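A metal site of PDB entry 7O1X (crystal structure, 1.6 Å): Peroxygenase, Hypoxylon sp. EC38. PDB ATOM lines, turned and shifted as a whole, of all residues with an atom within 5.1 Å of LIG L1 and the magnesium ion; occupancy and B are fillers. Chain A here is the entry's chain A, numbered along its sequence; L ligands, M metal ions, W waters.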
ATOM      1  N   PRO A  38      14.419  -7.315 -26.266  1.00  0.00           N
ATOM      2  CA  PRO A  38      13.258  -8.040 -25.762  1.00  0.00           C
ATOM      3  C   PRO A  38      12.008  -7.879 -26.634  1.00  0.00           C
ATOM      4  O   PRO A  38      10.952  -8.413 -26.288  1.00  0.00           O
ATOM      5  CB  PRO A  38      13.012  -7.425 -24.376  1.00  0.00           C
ATOM      6  CG  PRO A  38      13.806  -6.198 -24.347  1.00  0.00           C
ATOM      7  CD  PRO A  38      14.646  -6.052 -25.574  1.00  0.00           C
ATOM      8  N   CYS A  39      12.131  -7.159 -27.734  1.00  0.00           N
ATOM      9  CA  CYS A  39      11.030  -6.882 -28.687  1.00  0.00           C
ATOM     10  C   CYS A  39      11.039  -7.944 -29.773  1.00  0.00           C
ATOM     11  O   CYS A  39      11.978  -8.055 -30.570  1.00  0.00           O
ATOM     12  CB  CYS A  39      11.178  -5.535 -29.299  1.00  0.00           C
ATOM     13  SG  CYS A  39       9.812  -5.229 -30.448  1.00  0.00           S
ATOM     14  N   PRO A  40      10.000  -8.813 -29.841  1.00  0.00           N
ATOM     15  CA  PRO A  40       9.969  -9.819 -30.899  1.00  0.00           C
ATOM     16  C   PRO A  40       9.932  -9.203 -32.280  1.00  0.00           C
ATOM     17  O   PRO A  40      10.498  -9.822 -33.192  1.00  0.00           O
ATOM     18  CB  PRO A  40       8.688 -10.564 -30.642  1.00  0.00           C
ATOM     19  CG  PRO A  40       7.799  -9.558 -29.895  1.00  0.00           C
ATOM     20  CD  PRO A  40       8.747  -8.745 -29.033  1.00  0.00           C
ATOM     21  N   MET A  41       9.363  -8.016 -32.411  1.00  0.00           N
ATOM     22  CA  MET A  41       9.232  -7.434 -33.774  1.00  0.00           C
ATOM     23  C   MET A  41      10.554  -6.822 -34.216  1.00  0.00           C
ATOM     24  O   MET A  41      10.974  -7.052 -35.361  1.00  0.00           O
ATOM     25  CB  MET A  41       8.082  -6.435 -33.892  1.00  0.00           C
ATOM     26  CG  MET A  41       7.906  -5.858 -35.305  1.00  0.00           C
ATOM     27  SD  MET A  41       7.709  -7.161 -36.571  1.00  0.00           S
ATOM     28  CE  MET A  41       5.935  -7.431 -36.494  1.00  0.00           C
ATOM     29  N   LEU A  42      11.187  -5.999 -33.386  1.00  0.00           N
ATOM     30  CA  LEU A  42      12.497  -5.482 -33.840  1.00  0.00           C
ATOM     31  C   LEU A  42      13.482  -6.615 -34.099  1.00  0.00           C
ATOM     32  O   LEU A  42      14.266  -6.506 -35.053  1.00  0.00           O
ATOM     33  CB  LEU A  42      13.061  -4.514 -32.822  1.00  0.00           C
ATOM     34  CG  LEU A  42      12.230  -3.277 -32.594  1.00  0.00           C
ATOM     35  CD1 LEU A  42      13.029  -2.336 -31.697  1.00  0.00           C
ATOM     36  CD2 LEU A  42      11.809  -2.594 -33.864  1.00  0.00           C
ATOM     37  N   THR A  63      14.952   3.711 -38.531  1.00  0.00           N
ATOM     38  CA  THR A  63      13.730   3.235 -37.845  1.00  0.00           C
ATOM     39  C   THR A  63      12.513   3.548 -38.750  1.00  0.00           C
ATOM     40  O   THR A  63      11.683   2.668 -39.038  1.00  0.00           O
ATOM     41  CB  THR A  63      13.608   3.849 -36.457  1.00  0.00           C
ATOM     42  OG1 THR A  63      14.783   3.504 -35.709  1.00  0.00           O
ATOM     43  CG2 THR A  63      12.358   3.367 -35.778  1.00  0.00           C
ATOM     44  N   LEU A  67      10.472   0.354 -40.372  1.00  0.00           N
ATOM     45  CA  LEU A  67       9.101   0.098 -39.903  1.00  0.00           C
ATOM     46  C   LEU A  67       8.120   0.444 -41.024  1.00  0.00           C
ATOM     47  O   LEU A  67       7.109  -0.247 -41.156  1.00  0.00           O
ATOM     48  CB  LEU A  67       8.786   0.965 -38.679  1.00  0.00           C
ATOM     49  CG  LEU A  67       9.528   0.640 -37.417  1.00  0.00           C
ATOM     50  CD1 LEU A  67       9.043   1.385 -36.215  1.00  0.00           C
ATOM     51  CD2 LEU A  67       9.562  -0.766 -37.138  1.00  0.00           C
ATOM     52  N   LEU A  71       6.203  -2.898 -42.455  1.00  0.00           N
ATOM     53  CA  LEU A  71       4.918  -3.020 -41.693  1.00  0.00           C
ATOM     54  C   LEU A  71       3.988  -1.866 -42.017  1.00  0.00           C
ATOM     55  O   LEU A  71       2.876  -1.866 -41.525  1.00  0.00           O
ATOM     56  CB  LEU A  71       5.212  -3.041 -40.190  1.00  0.00           C
ATOM     57  CG  LEU A  71       6.107  -4.161 -39.678  1.00  0.00           C
ATOM     58  CD1 LEU A  71       6.413  -3.933 -38.220  1.00  0.00           C
ATOM     59  CD2 LEU A  71       5.431  -5.523 -39.890  1.00  0.00           C
ATOM     60  N   ILE A  73       4.256   1.139 -40.808  1.00  0.00           N
ATOM     61  CA  ILE A  73       4.151   2.037 -39.645  1.00  0.00           C
ATOM     62  C   ILE A  73       4.414   3.460 -40.142  1.00  0.00           C
ATOM     63  O   ILE A  73       5.366   3.636 -40.906  1.00  0.00           O
ATOM     64  CB  ILE A  73       5.028   1.559 -38.486  1.00  0.00           C
ATOM     65  CG1 ILE A  73       4.447   0.188 -38.032  1.00  0.00           C
ATOM     66  CG2 ILE A  73       5.015   2.614 -37.379  1.00  0.00           C
ATOM     67  CD1 ILE A  73       5.191  -0.414 -37.021  1.00  0.00           C
ATOM     68  N   LEU A  81       8.529   6.067 -31.368  1.00  0.00           N
ATOM     69  CA  LEU A  81       9.143   4.850 -30.811  1.00  0.00           C
ATOM     70  C   LEU A  81      10.656   5.018 -30.737  1.00  0.00           C
ATOM     71  O   LEU A  81      11.314   4.573 -29.749  1.00  0.00           O
ATOM     72  CB  LEU A  81       8.731   3.648 -31.667  1.00  0.00           C
ATOM     73  CG  LEU A  81       7.231   3.350 -31.640  1.00  0.00           C
ATOM     74  CD1 LEU A  81       6.839   2.322 -32.687  1.00  0.00           C
ATOM     75  CD2 LEU A  81       6.898   2.873 -30.254  1.00  0.00           C
ATOM     76  N   PHE A  82      11.221   5.598 -31.780  1.00  0.00           N
ATOM     77  CA  PHE A  82      12.674   5.845 -31.799  1.00  0.00           C
ATOM     78  C   PHE A  82      13.061   6.701 -30.586  1.00  0.00           C
ATOM     79  O   PHE A  82      14.080   6.385 -29.935  1.00  0.00           O
ATOM     80  CB  PHE A  82      13.134   6.512 -33.106  1.00  0.00           C
ATOM     81  CG  PHE A  82      14.592   6.876 -32.983  1.00  0.00           C
ATOM     82  CD1 PHE A  82      15.568   5.919 -33.286  1.00  0.00           C
ATOM     83  CD2 PHE A  82      14.993   8.120 -32.508  1.00  0.00           C
ATOM     84  CE1 PHE A  82      16.902   6.168 -33.054  1.00  0.00           C
ATOM     85  CE2 PHE A  82      16.338   8.375 -32.333  1.00  0.00           C
ATOM     86  CZ  PHE A  82      17.274   7.390 -32.548  1.00  0.00           C
ATOM     87  N   ALA A  85      13.337   4.554 -27.641  1.00  0.00           N
ATOM     88  CA  ALA A  85      14.451   3.625 -27.825  1.00  0.00           C
ATOM     89  C   ALA A  85      15.759   4.338 -27.456  1.00  0.00           C
ATOM     90  O   ALA A  85      16.621   3.733 -26.779  1.00  0.00           O
ATOM     91  CB  ALA A  85      14.457   3.060 -29.228  1.00  0.00           C
ATOM     92  N   PHE A  97      20.433   3.770 -31.221  1.00  0.00           N
ATOM     93  CA  PHE A  97      20.438   2.708 -30.184  1.00  0.00           C
ATOM     94  C   PHE A  97      20.812   1.400 -30.833  1.00  0.00           C
ATOM     95  O   PHE A  97      20.738   1.236 -32.025  1.00  0.00           O
ATOM     96  CB  PHE A  97      19.100   2.598 -29.449  1.00  0.00           C
ATOM     97  CG  PHE A  97      17.984   2.059 -30.296  1.00  0.00           C
ATOM     98  CD1 PHE A  97      17.381   2.869 -31.257  1.00  0.00           C
ATOM     99  CD2 PHE A  97      17.575   0.738 -30.196  1.00  0.00           C
ATOM    100  CE1 PHE A  97      16.356   2.387 -32.062  1.00  0.00           C
ATOM    101  CE2 PHE A  97      16.546   0.248 -31.004  1.00  0.00           C
ATOM    102  CZ  PHE A  97      15.938   1.069 -31.958  1.00  0.00           C
ATOM    103  N   LEU A 102      17.810  -1.966 -25.401  1.00  0.00           N
ATOM    104  CA  LEU A 102      16.367  -2.067 -25.086  1.00  0.00           C
ATOM    105  C   LEU A 102      16.122  -3.048 -23.954  1.00  0.00           C
ATOM    106  O   LEU A 102      15.077  -2.968 -23.332  1.00  0.00           O
ATOM    107  CB  LEU A 102      15.587  -2.473 -26.332  1.00  0.00           C
ATOM    108  CG  LEU A 102      15.504  -1.449 -27.474  1.00  0.00           C
ATOM    109  CD1 LEU A 102      14.700  -2.058 -28.600  1.00  0.00           C
ATOM    110  CD2 LEU A 102      14.961  -0.101 -27.016  1.00  0.00           C
ATOM    111  N   LEU A 108      12.701   0.810 -20.635  1.00  0.00           N
ATOM    112  CA  LEU A 108      11.500   0.432 -21.399  1.00  0.00           C
ATOM    113  C   LEU A 108      11.134  -0.995 -21.063  1.00  0.00           C
ATOM    114  O   LEU A 108       9.929  -1.291 -20.925  1.00  0.00           O
ATOM    115  CB  LEU A 108      11.730   0.579 -22.899  1.00  0.00           C
ATOM    116  CG  LEU A 108      12.209   1.933 -23.395  1.00  0.00           C
ATOM    117  CD1 LEU A 108      12.361   1.891 -24.917  1.00  0.00           C
ATOM    118  CD2 LEU A 108      11.282   3.065 -22.942  1.00  0.00           C
ATOM    119  N   GLU A 109      12.118  -1.863 -20.927  1.00  0.00           N
ATOM    120  CA  GLU A 109      11.839  -3.277 -20.607  1.00  0.00           C
ATOM    121  C   GLU A 109      11.124  -3.331 -19.259  1.00  0.00           C
ATOM    122  O   GLU A 109      11.496  -2.575 -18.304  1.00  0.00           O
ATOM    123  CB  GLU A 109      13.107  -4.114 -20.677  1.00  0.00           C
ATOM    124  CG  GLU A 109      12.884  -5.609 -20.542  1.00  0.00           C
ATOM    125  CD  GLU A 109      12.620  -6.154 -19.127  1.00  0.00           C
ATOM    126  OE1 GLU A 109      13.338  -5.691 -18.207  1.00  0.00           O
ATOM    127  OE2 GLU A 109      11.678  -6.969 -18.948  1.00  0.00           O
ATOM    128  N   HIS A 110      10.139  -4.194 -19.174  1.00  0.00           N
ATOM    129  CA  HIS A 110       9.272  -4.297 -17.964  1.00  0.00           C
ATOM    130  C   HIS A 110       8.883  -5.741 -17.644  1.00  0.00           C
ATOM    131  O   HIS A 110       8.934  -6.660 -18.491  1.00  0.00           O
ATOM    132  CB  HIS A 110       8.001  -3.445 -18.129  1.00  0.00           C
ATOM    133  CG  HIS A 110       7.243  -3.814 -19.349  1.00  0.00           C
ATOM    134  ND1 HIS A 110       6.397  -4.924 -19.372  1.00  0.00           N
ATOM    135  CD2 HIS A 110       7.173  -3.206 -20.586  1.00  0.00           C
ATOM    136  CE1 HIS A 110       5.902  -4.997 -20.584  1.00  0.00           C
ATOM    137  NE2 HIS A 110       6.347  -3.993 -21.337  1.00  0.00           N
ATOM    138  N   ASP A 111       8.589  -5.944 -16.366  1.00  0.00           N
ATOM    139  CA  ASP A 111       8.003  -7.202 -15.896  1.00  0.00           C
ATOM    140  C   ASP A 111       6.685  -7.506 -16.591  1.00  0.00           C
ATOM    141  O   ASP A 111       6.061  -6.636 -17.270  1.00  0.00           O
ATOM    142  CB  ASP A 111       7.835  -7.156 -14.391  1.00  0.00           C
ATOM    143  CG  ASP A 111       9.124  -7.027 -13.584  1.00  0.00           C
ATOM    144  OD1 ASP A 111      10.217  -7.419 -14.105  1.00  0.00           O
ATOM    145  OD2 ASP A 111       9.027  -6.511 -12.417  1.00  0.00           O
ATOM    146  N   SER A 113       6.009  -9.473 -19.083  1.00  0.00           N
ATOM    147  CA  SER A 113       6.081  -9.664 -20.525  1.00  0.00           C
ATOM    148  C   SER A 113       5.359 -10.965 -20.890  1.00  0.00           C
ATOM    149  O   SER A 113       5.227 -11.867 -20.058  1.00  0.00           O
ATOM    150  CB  SER A 113       7.515  -9.677 -21.071  1.00  0.00           C
ATOM    151  OG  SER A 113       8.211  -8.479 -20.800  1.00  0.00           O
ATOM    152  N   LEU A 114       4.844 -10.993 -22.131  1.00  0.00           N
ATOM    153  CA  LEU A 114       4.046 -12.146 -22.654  1.00  0.00           C
ATOM    154  C   LEU A 114       4.951 -13.343 -22.950  1.00  0.00           C
ATOM    155  O   LEU A 114       4.425 -14.477 -22.998  1.00  0.00           O
ATOM    156  CB  LEU A 114       3.326 -11.715 -23.912  1.00  0.00           C
ATOM    157  CG  LEU A 114       2.405 -10.505 -23.745  1.00  0.00           C
ATOM    158  CD1 LEU A 114       1.816 -10.125 -25.086  1.00  0.00           C
ATOM    159  CD2 LEU A 114       1.306 -10.738 -22.753  1.00  0.00           C
ATOM    160  N   SER A 115       6.226 -13.092 -23.292  1.00  0.00           N
ATOM    161  CA  SER A 115       7.062 -14.200 -23.871  1.00  0.00           C
ATOM    162  C   SER A 115       8.468 -14.199 -23.232  1.00  0.00           C
ATOM    163  O   SER A 115       9.285 -14.963 -23.705  1.00  0.00           O
ATOM    164  CB  SER A 115       7.197 -14.047 -25.390  1.00  0.00           C
ATOM    165  OG  SER A 115       7.976 -12.854 -25.723  1.00  0.00           O
ATOM    166  N   ARG A 116       8.739 -13.288 -22.308  1.00  0.00           N
ATOM    167  CA  ARG A 116      10.027 -13.142 -21.597  1.00  0.00           C
ATOM    168  C   ARG A 116       9.781 -13.323 -20.111  1.00  0.00           C
ATOM    169  O   ARG A 116       8.717 -12.928 -19.630  1.00  0.00           O
ATOM    170  CB  ARG A 116      10.725 -11.797 -21.805  1.00  0.00           C
ATOM    171  CG  ARG A 116      11.524 -11.720 -23.104  1.00  0.00           C
ATOM    172  CD  ARG A 116      10.812 -12.036 -24.389  1.00  0.00           C
ATOM    173  NE  ARG A 116      11.746 -11.836 -25.484  1.00  0.00           N
ATOM    174  CZ  ARG A 116      11.585 -12.227 -26.740  1.00  0.00           C
ATOM    175  NH1 ARG A 116      10.457 -12.838 -27.077  1.00  0.00           N
ATOM    176  NH2 ARG A 116      12.581 -12.071 -27.653  1.00  0.00           N
ATOM    177  N   GLN A 117      10.746 -13.933 -19.427  1.00  0.00           N
ATOM    178  CA  GLN A 117      10.703 -13.910 -17.954  1.00  0.00           C
ATOM    179  C   GLN A 117      11.006 -12.498 -17.458  1.00  0.00           C
ATOM    180  O   GLN A 117      11.725 -11.740 -18.075  1.00  0.00           O
ATOM    181  CB  GLN A 117      11.605 -15.010 -17.386  1.00  0.00           C
ATOM    182  CG  GLN A 117      13.054 -14.705 -17.512  1.00  0.00           C
ATOM    183  CD  GLN A 117      13.937 -15.940 -17.429  1.00  0.00           C
ATOM    184  OE1 GLN A 117      13.682 -16.900 -16.630  1.00  0.00           O
ATOM    185  NE2 GLN A 117      15.009 -15.897 -18.212  1.00  0.00           N
ATOM    186  N   ALA A 124      15.827 -11.099 -19.326  1.00  0.00           N
ATOM    187  CA  ALA A 124      14.486 -10.661 -19.785  1.00  0.00           C
ATOM    188  C   ALA A 124      14.514 -10.285 -21.263  1.00  0.00           C
ATOM    189  O   ALA A 124      13.587  -9.631 -21.724  1.00  0.00           O
ATOM    190  CB  ALA A 124      14.008  -9.514 -18.940  1.00  0.00           C
ATOM    191  N   PHE A 176       3.551   0.871 -22.145  1.00  0.00           N
ATOM    192  CA  PHE A 176       4.243  -0.049 -23.075  1.00  0.00           C
ATOM    193  C   PHE A 176       3.460  -1.370 -23.087  1.00  0.00           C
ATOM    194  O   PHE A 176       3.184  -1.858 -24.145  1.00  0.00           O
ATOM    195  CB  PHE A 176       5.725  -0.252 -22.748  1.00  0.00           C
ATOM    196  CG  PHE A 176       6.638   0.565 -23.592  1.00  0.00           C
ATOM    197  CD1 PHE A 176       6.538   1.960 -23.536  1.00  0.00           C
ATOM    198  CD2 PHE A 176       7.609  -0.038 -24.437  1.00  0.00           C
ATOM    199  CE1 PHE A 176       7.384   2.720 -24.335  1.00  0.00           C
ATOM    200  CE2 PHE A 176       8.438   0.760 -25.223  1.00  0.00           C
ATOM    201  CZ  PHE A 176       8.321   2.125 -25.132  1.00  0.00           C
ATOM    202  N   GLU A 180       1.866  -2.944 -26.367  1.00  0.00           N
ATOM    203  CA  GLU A 180       2.495  -4.110 -27.052  1.00  0.00           C
ATOM    204  C   GLU A 180       1.383  -5.076 -27.465  1.00  0.00           C
ATOM    205  O   GLU A 180       1.450  -5.640 -28.535  1.00  0.00           O
ATOM    206  CB  GLU A 180       3.465  -4.790 -26.116  1.00  0.00           C
ATOM    207  CG  GLU A 180       4.670  -3.935 -25.774  1.00  0.00           C
ATOM    208  CD  GLU A 180       5.255  -4.107 -24.355  1.00  0.00           C
ATOM    209  OE1 GLU A 180       4.858  -5.031 -23.653  1.00  0.00           O
ATOM    210  OE2 GLU A 180       6.077  -3.239 -23.943  1.00  0.00           O
ATOM    211  N   ALA A 183      -0.295  -3.588 -30.367  1.00  0.00           N
ATOM    212  CA  ALA A 183       0.577  -3.652 -31.551  1.00  0.00           C
ATOM    213  C   ALA A 183       0.444  -5.004 -32.279  1.00  0.00           C
ATOM    214  O   ALA A 183       0.321  -5.026 -33.500  1.00  0.00           O
ATOM    215  CB  ALA A 183       2.021  -3.401 -31.136  1.00  0.00           C
ATOM    216  N   TYR A 184       0.507  -6.107 -31.557  1.00  0.00           N
ATOM    217  CA  TYR A 184       0.459  -7.425 -32.265  1.00  0.00           C
ATOM    218  C   TYR A 184      -0.874  -7.572 -32.978  1.00  0.00           C
ATOM    219  O   TYR A 184      -0.923  -8.136 -34.029  1.00  0.00           O
ATOM    220  CB  TYR A 184       0.930  -8.604 -31.432  1.00  0.00           C
ATOM    221  CG  TYR A 184       0.014  -9.109 -30.364  1.00  0.00           C
ATOM    222  CD1 TYR A 184      -1.110  -9.849 -30.678  1.00  0.00           C
ATOM    223  CD2 TYR A 184       0.391  -9.045 -29.023  1.00  0.00           C
ATOM    224  CE1 TYR A 184      -1.904 -10.369 -29.661  1.00  0.00           C
ATOM    225  CE2 TYR A 184      -0.380  -9.581 -28.020  1.00  0.00           C
ATOM    226  CZ  TYR A 184      -1.536 -10.267 -28.343  1.00  0.00           C
ATOM    227  OH  TYR A 184      -2.327 -10.795 -27.366  1.00  0.00           O
ATOM    228  N   ILE A 187      -0.841  -4.345 -35.894  1.00  0.00           N
ATOM    229  CA  ILE A 187       0.262  -4.311 -36.865  1.00  0.00           C
ATOM    230  C   ILE A 187       0.349  -5.638 -37.623  1.00  0.00           C
ATOM    231  O   ILE A 187       0.594  -5.615 -38.834  1.00  0.00           O
ATOM    232  CB  ILE A 187       1.552  -3.888 -36.111  1.00  0.00           C
ATOM    233  CG1 ILE A 187       1.442  -2.403 -35.715  1.00  0.00           C
ATOM    234  CG2 ILE A 187       2.734  -4.186 -36.999  1.00  0.00           C
ATOM    235  CD1 ILE A 187       2.487  -1.819 -34.721  1.00  0.00           C
ATOM    236  N   LEU A 204       5.459 -15.355 -35.092  1.00  0.00           N
ATOM    237  CA  LEU A 204       6.349 -14.213 -34.853  1.00  0.00           C
ATOM    238  C   LEU A 204       7.156 -14.457 -33.576  1.00  0.00           C
ATOM    239  O   LEU A 204       8.359 -14.256 -33.567  1.00  0.00           O
ATOM    240  CB  LEU A 204       5.502 -12.964 -34.753  1.00  0.00           C
ATOM    241  CG  LEU A 204       6.367 -11.699 -34.583  1.00  0.00           C
ATOM    242  CD1 LEU A 204       6.850 -11.208 -35.919  1.00  0.00           C
ATOM    243  CD2 LEU A 204       5.637 -10.581 -33.863  1.00  0.00           C
ATOM    244  N   PHE A 205       6.487 -14.749 -32.482  1.00  0.00           N
ATOM    245  CA  PHE A 205       7.187 -14.926 -31.188  1.00  0.00           C
ATOM    246  C   PHE A 205       8.174 -16.088 -31.231  1.00  0.00           C
ATOM    247  O   PHE A 205       9.313 -15.947 -30.739  1.00  0.00           O
ATOM    248  CB  PHE A 205       6.192 -15.075 -30.062  1.00  0.00           C
ATOM    249  CG  PHE A 205       5.604 -13.816 -29.536  1.00  0.00           C
ATOM    250  CD1 PHE A 205       4.459 -13.264 -30.042  1.00  0.00           C
ATOM    251  CD2 PHE A 205       6.201 -13.178 -28.469  1.00  0.00           C
ATOM    252  CE1 PHE A 205       3.901 -12.138 -29.455  1.00  0.00           C
ATOM    253  CE2 PHE A 205       5.688 -12.018 -27.933  1.00  0.00           C
ATOM    254  CZ  PHE A 205       4.473 -11.549 -28.384  1.00  0.00           C
HETATM  255  C1  LIG L   1       8.061  -5.593 -26.576  1.00  0.00           C
HETATM  256  C2  LIG L   1      10.517  -1.705 -27.927  1.00  0.00           C
HETATM  257  C3  LIG L   1       8.394  -1.855 -32.255  1.00  0.00           C
HETATM  258  C4  LIG L   1       5.613  -5.564 -30.761  1.00  0.00           C
HETATM  259  C5  LIG L   1       8.977  -4.573 -26.617  1.00  0.00           C
HETATM  260  C6  LIG L   1       9.892  -4.270 -25.565  1.00  0.00           C
HETATM  261  C7  LIG L   1      10.599  -3.176 -25.920  1.00  0.00           C
HETATM  262  C8  LIG L   1      10.119  -2.799 -27.210  1.00  0.00           C
HETATM  263  C9  LIG L   1      11.617  -2.401 -25.131  1.00  0.00           C
HETATM  264  C10 LIG L   1      10.039  -5.050 -24.287  1.00  0.00           C
HETATM  265  C11 LIG L   1       8.964  -4.762 -23.270  1.00  0.00           C
HETATM  266  C12 LIG L   1       8.874  -5.875 -22.316  1.00  0.00           C
HETATM  267  O1  LIG L   1       8.072  -6.839 -22.692  1.00  0.00           O
HETATM  268  O2  LIG L   1       9.538  -6.035 -21.283  1.00  0.00           O
HETATM  269  C13 LIG L   1      10.073  -1.389 -29.224  1.00  0.00           C
HETATM  270  C14 LIG L   1      10.581  -0.269 -29.990  1.00  0.00           C
HETATM  271  C15 LIG L   1      10.053  -0.318 -31.192  1.00  0.00           C
HETATM  272  C16 LIG L   1       9.143  -1.491 -31.187  1.00  0.00           C
HETATM  273  C17 LIG L   1      11.567   0.757 -29.490  1.00  0.00           C
HETATM  274  C18 LIG L   1      10.252   0.525 -32.362  1.00  0.00           C
HETATM  275  C19 LIG L   1      11.297   1.350 -32.598  1.00  0.00           C
HETATM  276  C20 LIG L   1       7.422  -2.891 -32.254  1.00  0.00           C
HETATM  277  C21 LIG L   1       6.514  -3.245 -33.278  1.00  0.00           C
HETATM  278  C22 LIG L   1       5.748  -4.253 -32.862  1.00  0.00           C
HETATM  279  C23 LIG L   1       6.182  -4.561 -31.512  1.00  0.00           C
HETATM  280  C24 LIG L   1       6.489  -2.479 -34.605  1.00  0.00           C
HETATM  281  C25 LIG L   1       4.737  -4.837 -33.691  1.00  0.00           C
HETATM  282  C26 LIG L   1       4.135  -5.971 -33.650  1.00  0.00           C
HETATM  283  C27 LIG L   1       6.072  -5.841 -29.459  1.00  0.00           C
HETATM  284  C28 LIG L   1       5.460  -6.868 -28.629  1.00  0.00           C
HETATM  285  C29 LIG L   1       6.108  -6.933 -27.460  1.00  0.00           C
HETATM  286  C30 LIG L   1       7.170  -5.863 -27.593  1.00  0.00           C
HETATM  287  C31 LIG L   1       4.281  -7.698 -29.034  1.00  0.00           C
HETATM  288  C32 LIG L   1       5.844  -7.711 -26.227  1.00  0.00           C
HETATM  289  C33 LIG L   1       6.846  -8.860 -26.001  1.00  0.00           C
HETATM  290  C34 LIG L   1       6.504  -9.672 -24.766  1.00  0.00           C
HETATM  291  O3  LIG L   1       7.044 -10.755 -24.537  1.00  0.00           O
HETATM  292  O4  LIG L   1       5.645  -9.200 -23.961  1.00  0.00           O
HETATM  293  N1  LIG L   1       9.128  -3.704 -27.622  1.00  0.00           N
HETATM  294  N2  LIG L   1       9.205  -2.047 -29.954  1.00  0.00           N
HETATM  295  N3  LIG L   1       7.249  -3.673 -31.175  1.00  0.00           N
HETATM  296  N4  LIG L   1       7.077  -5.218 -28.805  1.00  0.00           N
HETATM  297 FE1  LIG L   1       8.232  -3.753 -29.438  1.00  0.00          FE
HETATM  298  N1  LG2 L   2       5.450  -0.636 -28.089  1.00  0.00           N
HETATM  299  C1  LG2 L   2       6.685  -1.201 -28.006  1.00  0.00           C
HETATM  300  N2  LG2 L   2       6.585  -2.364 -28.712  1.00  0.00           N
HETATM  301  C2  LG2 L   2       5.236  -2.379 -29.153  1.00  0.00           C
HETATM  302  C3  LG2 L   2       4.566  -1.223 -28.858  1.00  0.00           C
HETATM  303  C4  LG2 L   2       5.160   0.531 -27.513  1.00  0.00           C
HETATM  304  C5  LG2 L   2       3.923   0.696 -26.844  1.00  0.00           C
HETATM  305  C6  LG2 L   2       3.558   1.946 -26.240  1.00  0.00           C
HETATM  306  C7  LG2 L   2       4.446   3.049 -26.219  1.00  0.00           C
HETATM  307  C8  LG2 L   2       5.694   2.892 -26.863  1.00  0.00           C
HETATM  308  C9  LG2 L   2       6.043   1.627 -27.471  1.00  0.00           C
HETATM  309 MG    MG M   1       9.963  -7.666 -19.981  1.00  0.00          MG
HETATM  310  O   HOH W   1       9.830  -8.879 -23.859  1.00  0.00           O
HETATM  311  O   HOH W   2      11.108  -8.536 -21.534  1.00  0.00           O
HETATM  312  O   HOH W   3      10.157  -9.354 -18.732  1.00  0.00           O
HETATM  313  O   HOH W   4       3.783  -7.303 -23.422  1.00  0.00           O
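Of the 31 residues printed, 3 come within 4 Å of the magnesium ion. The nearest printed residue that does not touch the magnesium ion is Asp 111 (4.2 Å).
N of His 110 sits close to O2 of LIG L1 (2.9 Å). An iron atom (FE1) of LIG L1 is bound by the side-chain sulfur (SG) of Cys 39, at 2.4 Å. The backbone NH of Ser 115 sits at hydrogen-bond distance from an oxygen (O3) of LIG L1, 2.8 Å away. OG of Ser 115 sits at hydrogen-bond distance from O3 of LIG L1 (2.6 Å). The backbone NH of Leu 114 sits at hydrogen-bond distance from an oxygen (O4) of LIG L1, 2.7 Å away.
Water W4 lies within hydrogen-bond range of OE1 of Glu 180 and O4 of LIG L1. Water W1 bridges the backbone carbonyl oxygen of Pro 38 (2.7 Å) and an oxygen (O1) of LIG L1 (2.9 Å).
An iron atom (FE1) of LIG L1 is bound by a nitrogen (N2) of LG2 L2 (2.3 Å).
Pro 38 touches LIG L1. Pro 40 touches LIG L1. Met 41 touches LIG L1. Leu 42 touches LIG L1. Thr 63 touches LIG L1 (CG2 to C19, 3.9 Å). CD1 of Leu 71 touches C24 of LIG L1, 3.9 Å away. Ile 73 touches LIG L1. Leu 81 touches LIG L1 (CB to C18, 3.5 Å). Ala 85 touches LIG L1 (CB to C17, 3.7 Å). O of Leu 102 touches C9 of LIG L1 (3.9 Å). Leu 108 touches LIG L1 (CB to C9, 3.7 Å). Arg 116 touches LIG L1. Glu 180 touches LIG L1. Ala 183 touches LIG L1 (O to C26, 3.9 Å). CD1 of Ile 187 touches C25 of LIG L1, 3.9 Å away. Phe 205 touches LIG L1 (CE2 to O3, 3.9 Å). Within 4 Å of LIG L1: Pro 38, Cys 39, Pro 40, Met 41, Leu 42, Thr 63, Leu 71, Ile 73, Leu 81, Ala 85, Leu 102, Leu 108, Glu 109, His 110, Ser 113, Leu 114, Ser 115, Arg 116, Glu 180, Ala 183, Ile 187 and Phe 205.
The magnesium ion is bound by the backbone carbonyl oxygen (O) of His 110 (2.1 Å), the side-chain hydroxyl (OG) of Ser 113 (2.1 Å), water W3 (2.1 Å), water W2 (2.1 Å), the side-chain carboxylate (OE2) of Glu 109 (2.1 Å) and an oxygen (O2) of LIG L1 (2.1 Å).
The side-chain carboxylate (OE2) of Glu 180 lies within hydrogen-bond range of a ring nitrogen (NE2) of His 110, 2.7 Å away. SG of Cys 39 lies close to N of Met 41, 3.4 Å away. N of Leu 42 sits close to SG of Cys 39, 3.3 Å away. The side-chain hydroxyl (OG) of Ser 115 lies within hydrogen-bond range of the guanidinium group (NH1) of Arg 116. O of Leu 67 sits at hydrogen-bond distance from N of Ile 73, at 3.2 Å.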
